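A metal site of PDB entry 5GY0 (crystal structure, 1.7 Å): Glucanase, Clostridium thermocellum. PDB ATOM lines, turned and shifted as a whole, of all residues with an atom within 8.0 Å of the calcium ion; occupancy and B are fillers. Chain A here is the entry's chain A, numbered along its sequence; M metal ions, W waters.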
ATOM      1  N   THR A 461      10.376  13.649   7.722  1.00  0.00           N
ATOM      2  CA  THR A 461      10.902  14.630   8.653  1.00  0.00           C
ATOM      3  C   THR A 461      12.413  14.570   8.548  1.00  0.00           C
ATOM      4  O   THR A 461      12.979  13.483   8.604  1.00  0.00           O
ATOM      5  CB  THR A 461      10.534  14.241  10.097  1.00  0.00           C
ATOM      6  OG1 THR A 461       9.112  14.336  10.264  1.00  0.00           O
ATOM      7  CG2 THR A 461      11.241  15.142  11.091  1.00  0.00           C
ATOM      8  N   TYR A 486      12.146   9.543  19.137  1.00  0.00           N
ATOM      9  CA  TYR A 486      10.924   8.734  19.231  1.00  0.00           C
ATOM     10  C   TYR A 486       9.828   9.233  18.306  1.00  0.00           C
ATOM     11  O   TYR A 486       9.595  10.442  18.187  1.00  0.00           O
ATOM     12  CB  TYR A 486      10.369   8.745  20.664  1.00  0.00           C
ATOM     13  CG  TYR A 486      11.332   8.226  21.693  1.00  0.00           C
ATOM     14  CD1 TYR A 486      11.397   6.859  21.977  1.00  0.00           C
ATOM     15  CD2 TYR A 486      12.199   9.088  22.368  1.00  0.00           C
ATOM     16  CE1 TYR A 486      12.301   6.362  22.926  1.00  0.00           C
ATOM     17  CE2 TYR A 486      13.085   8.607  23.312  1.00  0.00           C
ATOM     18  CZ  TYR A 486      13.133   7.256  23.590  1.00  0.00           C
ATOM     19  OH  TYR A 486      14.022   6.788  24.528  1.00  0.00           O
ATOM     20  N   MET A 487       9.139   8.286  17.682  1.00  0.00           N
ATOM     21  CA  MET A 487       8.052   8.599  16.778  1.00  0.00           C
ATOM     22  C   MET A 487       6.834   7.731  17.119  1.00  0.00           C
ATOM     23  O   MET A 487       6.982   6.697  17.757  1.00  0.00           O
ATOM     24  CB  MET A 487       8.499   8.374  15.329  1.00  0.00           C
ATOM     25  CG  MET A 487       8.974   6.968  14.971  1.00  0.00           C
ATOM     26  SD  MET A 487      10.187   7.122  13.629  1.00  0.00           S
ATOM     27  CE  MET A 487      11.695   6.838  14.545  1.00  0.00           C
ATOM     28  N   ASP A 488       5.665   8.173  16.684  1.00  0.00           N
ATOM     29  CA  ASP A 488       4.446   7.379  16.817  1.00  0.00           C
ATOM     30  C   ASP A 488       4.078   7.012  15.397  1.00  0.00           C
ATOM     31  O   ASP A 488       3.870   7.892  14.575  1.00  0.00           O
ATOM     32  CB  ASP A 488       3.342   8.222  17.454  1.00  0.00           C
ATOM     33  CG  ASP A 488       2.071   7.414  17.698  1.00  0.00           C
ATOM     34  OD1 ASP A 488       1.815   6.452  16.951  1.00  0.00           O
ATOM     35  OD2 ASP A 488       1.354   7.764  18.643  1.00  0.00           O
ATOM     36  N   LEU A 489       4.036   5.726  15.103  1.00  0.00           N
ATOM     37  CA  LEU A 489       3.731   5.249  13.760  1.00  0.00           C
ATOM     38  C   LEU A 489       2.280   4.850  13.543  1.00  0.00           C
ATOM     39  O   LEU A 489       1.969   4.184  12.556  1.00  0.00           O
ATOM     40  CB  LEU A 489       4.666   4.097  13.389  1.00  0.00           C
ATOM     41  CG  LEU A 489       6.156   4.442  13.456  1.00  0.00           C
ATOM     42  CD1 LEU A 489       6.983   3.270  12.941  1.00  0.00           C
ATOM     43  CD2 LEU A 489       6.492   5.711  12.680  1.00  0.00           C
ATOM     44  N   THR A 490       1.385   5.289  14.429  1.00  0.00           N
ATOM     45  CA  THR A 490      -0.027   4.938  14.266  1.00  0.00           C
ATOM     46  C   THR A 490      -0.555   5.240  12.859  1.00  0.00           C
ATOM     47  O   THR A 490      -1.225   4.400  12.257  1.00  0.00           O
ATOM     48  CB  THR A 490      -0.920   5.613  15.322  1.00  0.00           C
ATOM     49  OG1 THR A 490      -0.584   5.085  16.617  1.00  0.00           O
ATOM     50  CG2 THR A 490      -2.401   5.342  15.047  1.00  0.00           C
ATOM     51  N   GLU A 491      -0.240   6.423  12.327  1.00  0.00           N
ATOM     52  CA  GLU A 491      -0.738   6.836  11.010  1.00  0.00           C
ATOM     53  C   GLU A 491      -0.180   5.986   9.854  1.00  0.00           C
ATOM     54  O   GLU A 491      -0.828   5.854   8.806  1.00  0.00           O
ATOM     55  CB  GLU A 491      -0.507   8.331  10.794  1.00  0.00           C
ATOM     56  CG  GLU A 491       0.927   8.738  10.441  1.00  0.00           C
ATOM     57  CD  GLU A 491       1.856   8.961  11.628  1.00  0.00           C
ATOM     58  OE1 GLU A 491       1.422   8.808  12.795  1.00  0.00           O
ATOM     59  OE2 GLU A 491       3.036   9.298  11.395  1.00  0.00           O
ATOM     60  N   VAL A 492       1.006   5.428  10.060  1.00  0.00           N
ATOM     61  CA  VAL A 492       1.644   4.560   9.074  1.00  0.00           C
ATOM     62  C   VAL A 492       0.863   3.263   8.941  1.00  0.00           C
ATOM     63  O   VAL A 492       0.552   2.846   7.827  1.00  0.00           O
ATOM     64  CB  VAL A 492       3.095   4.228   9.471  1.00  0.00           C
ATOM     65  CG1 VAL A 492       3.752   3.291   8.458  1.00  0.00           C
ATOM     66  CG2 VAL A 492       3.904   5.504   9.618  1.00  0.00           C
ATOM     67  N   ASN A 526       2.431   1.741  19.520  1.00  0.00           N
ATOM     68  CA  ASN A 526       2.869   2.228  18.207  1.00  0.00           C
ATOM     69  C   ASN A 526       4.067   3.176  18.265  1.00  0.00           C
ATOM     70  O   ASN A 526       4.369   3.848  17.278  1.00  0.00           O
ATOM     71  CB  ASN A 526       1.696   2.853  17.435  1.00  0.00           C
ATOM     72  CG  ASN A 526       0.690   1.814  16.984  1.00  0.00           C
ATOM     73  OD1 ASN A 526       0.962   0.613  16.989  1.00  0.00           O
ATOM     74  ND2 ASN A 526      -0.486   2.273  16.588  1.00  0.00           N
ATOM     75  N   ILE A 527       4.740   3.211  19.405  1.00  0.00           N
ATOM     76  CA  ILE A 527       5.896   4.081  19.645  1.00  0.00           C
ATOM     77  C   ILE A 527       7.188   3.360  19.271  1.00  0.00           C
ATOM     78  O   ILE A 527       7.474   2.257  19.749  1.00  0.00           O
ATOM     79  CB  ILE A 527       5.972   4.570  21.109  1.00  0.00           C
ATOM     80  CG1 ILE A 527       4.687   5.269  21.560  1.00  0.00           C
ATOM     81  CG2 ILE A 527       7.209   5.439  21.342  1.00  0.00           C
ATOM     82  CD1 ILE A 527       4.072   6.216  20.539  1.00  0.00           C
ATOM     83  N   PHE A 564       0.526  10.278   4.282  1.00  0.00           N
ATOM     84  CA  PHE A 564       0.075   9.951   5.638  1.00  0.00           C
ATOM     85  C   PHE A 564       1.012  10.405   6.767  1.00  0.00           C
ATOM     86  O   PHE A 564       0.570  10.564   7.898  1.00  0.00           O
ATOM     87  CB  PHE A 564      -0.228   8.455   5.806  1.00  0.00           C
ATOM     88  CG  PHE A 564       0.934   7.560   5.485  1.00  0.00           C
ATOM     89  CD1 PHE A 564       1.971   7.374   6.394  1.00  0.00           C
ATOM     90  CD2 PHE A 564       0.983   6.892   4.268  1.00  0.00           C
ATOM     91  CE1 PHE A 564       3.045   6.556   6.110  1.00  0.00           C
ATOM     92  CE2 PHE A 564       2.056   6.072   3.962  1.00  0.00           C
ATOM     93  CZ  PHE A 564       3.084   5.888   4.871  1.00  0.00           C
ATOM     94  N   TRP A 565       2.294  10.572   6.449  1.00  0.00           N
ATOM     95  CA  TRP A 565       3.325  10.877   7.448  1.00  0.00           C
ATOM     96  C   TRP A 565       2.853  12.014   8.346  1.00  0.00           C
ATOM     97  O   TRP A 565       2.478  13.072   7.856  1.00  0.00           O
ATOM     98  CB  TRP A 565       4.640  11.274   6.771  1.00  0.00           C
ATOM     99  CG  TRP A 565       5.799  11.440   7.731  1.00  0.00           C
ATOM    100  CD1 TRP A 565       6.411  12.615   8.076  1.00  0.00           C
ATOM    101  CD2 TRP A 565       6.437  10.413   8.485  1.00  0.00           C
ATOM    102  NE1 TRP A 565       7.408  12.368   8.990  1.00  0.00           N
ATOM    103  CE2 TRP A 565       7.456  11.024   9.250  1.00  0.00           C
ATOM    104  CE3 TRP A 565       6.263   9.026   8.574  1.00  0.00           C
ATOM    105  CZ2 TRP A 565       8.280  10.302  10.114  1.00  0.00           C
ATOM    106  CZ3 TRP A 565       7.087   8.308   9.430  1.00  0.00           C
ATOM    107  CH2 TRP A 565       8.081   8.946  10.193  1.00  0.00           C
ATOM    108  N   ASP A 566       2.844  11.782   9.655  1.00  0.00           N
ATOM    109  CA  ASP A 566       2.388  12.768  10.622  1.00  0.00           C
ATOM    110  C   ASP A 566       3.422  12.903  11.736  1.00  0.00           C
ATOM    111  O   ASP A 566       3.475  12.060  12.641  1.00  0.00           O
ATOM    112  CB  ASP A 566       1.036  12.343  11.221  1.00  0.00           C
ATOM    113  CG  ASP A 566       0.461  13.412  12.118  1.00  0.00           C
ATOM    114  OD1 ASP A 566       1.064  14.501  12.223  1.00  0.00           O
ATOM    115  OD2 ASP A 566      -0.604  13.181  12.735  1.00  0.00           O
ATOM    116  N   PRO A 567       4.249  13.950  11.663  1.00  0.00           N
ATOM    117  CA  PRO A 567       5.243  14.092  12.723  1.00  0.00           C
ATOM    118  C   PRO A 567       4.649  14.716  13.990  1.00  0.00           C
ATOM    119  O   PRO A 567       5.276  14.670  15.053  1.00  0.00           O
ATOM    120  CB  PRO A 567       6.280  14.999  12.075  1.00  0.00           C
ATOM    121  CG  PRO A 567       5.491  15.866  11.163  1.00  0.00           C
ATOM    122  CD  PRO A 567       4.452  14.941  10.583  1.00  0.00           C
ATOM    123  N   THR A 568       3.442  15.267  13.889  1.00  0.00           N
ATOM    124  CA  THR A 568       2.852  15.988  15.024  1.00  0.00           C
ATOM    125  C   THR A 568       2.444  15.094  16.196  1.00  0.00           C
ATOM    126  O   THR A 568       2.221  15.587  17.300  1.00  0.00           O
ATOM    127  CB  THR A 568       1.685  16.917  14.602  1.00  0.00           C
ATOM    128  OG1 THR A 568       0.541  16.125  14.275  1.00  0.00           O
ATOM    129  CG2 THR A 568       2.056  17.774  13.402  1.00  0.00           C
ATOM    130  N   ASN A 569       2.360  13.785  15.976  1.00  0.00           N
ATOM    131  CA  ASN A 569       2.163  12.884  17.103  1.00  0.00           C
ATOM    132  C   ASN A 569       3.426  12.161  17.569  1.00  0.00           C
ATOM    133  O   ASN A 569       3.354  11.245  18.384  1.00  0.00           O
ATOM    134  CB  ASN A 569       1.025  11.890  16.836  1.00  0.00           C
ATOM    135  CG  ASN A 569       1.342  10.933  15.700  1.00  0.00           C
ATOM    136  OD1 ASN A 569       2.453  10.952  15.151  1.00  0.00           O
ATOM    137  ND2 ASN A 569       0.380  10.086  15.350  1.00  0.00           N
ATOM    138  N   ASP A 570       4.586  12.580  17.066  1.00  0.00           N
ATOM    139  CA  ASP A 570       5.869  11.978  17.442  1.00  0.00           C
ATOM    140  C   ASP A 570       6.468  12.704  18.641  1.00  0.00           C
ATOM    141  O   ASP A 570       6.624  13.919  18.633  1.00  0.00           O
ATOM    142  CB  ASP A 570       6.860  12.065  16.278  1.00  0.00           C
ATOM    143  CG  ASP A 570       6.406  11.298  15.037  1.00  0.00           C
ATOM    144  OD1 ASP A 570       5.387  10.558  15.062  1.00  0.00           O
ATOM    145  OD2 ASP A 570       7.086  11.455  13.993  1.00  0.00           O
ATOM    146  N   PHE A 571       6.787  11.926  19.672  1.00  0.00           N
ATOM    147  CA  PHE A 571       7.290  12.437  20.953  1.00  0.00           C
ATOM    148  C   PHE A 571       8.505  13.335  20.754  1.00  0.00           C
ATOM    149  O   PHE A 571       8.575  14.406  21.341  1.00  0.00           O
ATOM    150  CB  PHE A 571       7.649  11.250  21.843  1.00  0.00           C
ATOM    151  CG  PHE A 571       8.220  11.619  23.199  1.00  0.00           C
ATOM    152  CD1 PHE A 571       7.383  11.788  24.291  1.00  0.00           C
ATOM    153  CD2 PHE A 571       9.591  11.729  23.381  1.00  0.00           C
ATOM    154  CE1 PHE A 571       7.922  12.095  25.545  1.00  0.00           C
ATOM    155  CE2 PHE A 571      10.136  12.017  24.628  1.00  0.00           C
ATOM    156  CZ  PHE A 571       9.293  12.209  25.718  1.00  0.00           C
ATOM    157  N   TYR A 573       9.352  15.198  18.215  1.00  0.00           N
ATOM    158  CA  TYR A 573       9.102  16.370  17.368  1.00  0.00           C
ATOM    159  C   TYR A 573       8.522  17.538  18.186  1.00  0.00           C
ATOM    160  O   TYR A 573       8.475  18.670  17.723  1.00  0.00           O
ATOM    161  CB  TYR A 573       8.124  15.971  16.259  1.00  0.00           C
ATOM    162  CG  TYR A 573       8.056  16.817  15.009  1.00  0.00           C
ATOM    163  CD1 TYR A 573       9.071  16.789  14.059  1.00  0.00           C
ATOM    164  CD2 TYR A 573       6.926  17.591  14.732  1.00  0.00           C
ATOM    165  CE1 TYR A 573       8.975  17.522  12.881  1.00  0.00           C
ATOM    166  CE2 TYR A 573       6.833  18.347  13.553  1.00  0.00           C
ATOM    167  CZ  TYR A 573       7.844  18.285  12.632  1.00  0.00           C
ATOM    168  OH  TYR A 573       7.756  19.008  11.451  1.00  0.00           O
HETATM  169 CA    CA M   1       3.746   9.937  13.526  1.00  0.00          CA
HETATM  170  O   HOH W   1       5.769   9.770  12.346  1.00  0.00           O
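The calcium ion is bound by the backbone carbonyl oxygen (O) of Asp 488 (2.3 Å), the side-chain amide oxygen (OD1) of Asn 569 (2.3 Å), the backbone carbonyl oxygen (O) of Asp 566 (2.3 Å), the side-chain carboxylate (OD1) of Asp 570 (2.3 Å), the side-chain carboxylate (OE2) of Glu 491 (2.3 Å), water W1 (2.3 Å) and the side-chain carboxylate (OE1) of Glu 491 (2.7 Å).
The side-chain carboxylate (OD1) of Asp 566 lies within hydrogen-bond range of the side-chain hydroxyl (OG1) of Thr 568 (2.7 Å). OD1 of Asp 488 is in hydrogen-bond range of OG1 of Thr 490 (2.8 Å).
Within 4 Å of the calcium ion: Asp 488, Glu 491, Asp 566, Asn 569 and Asp 570.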
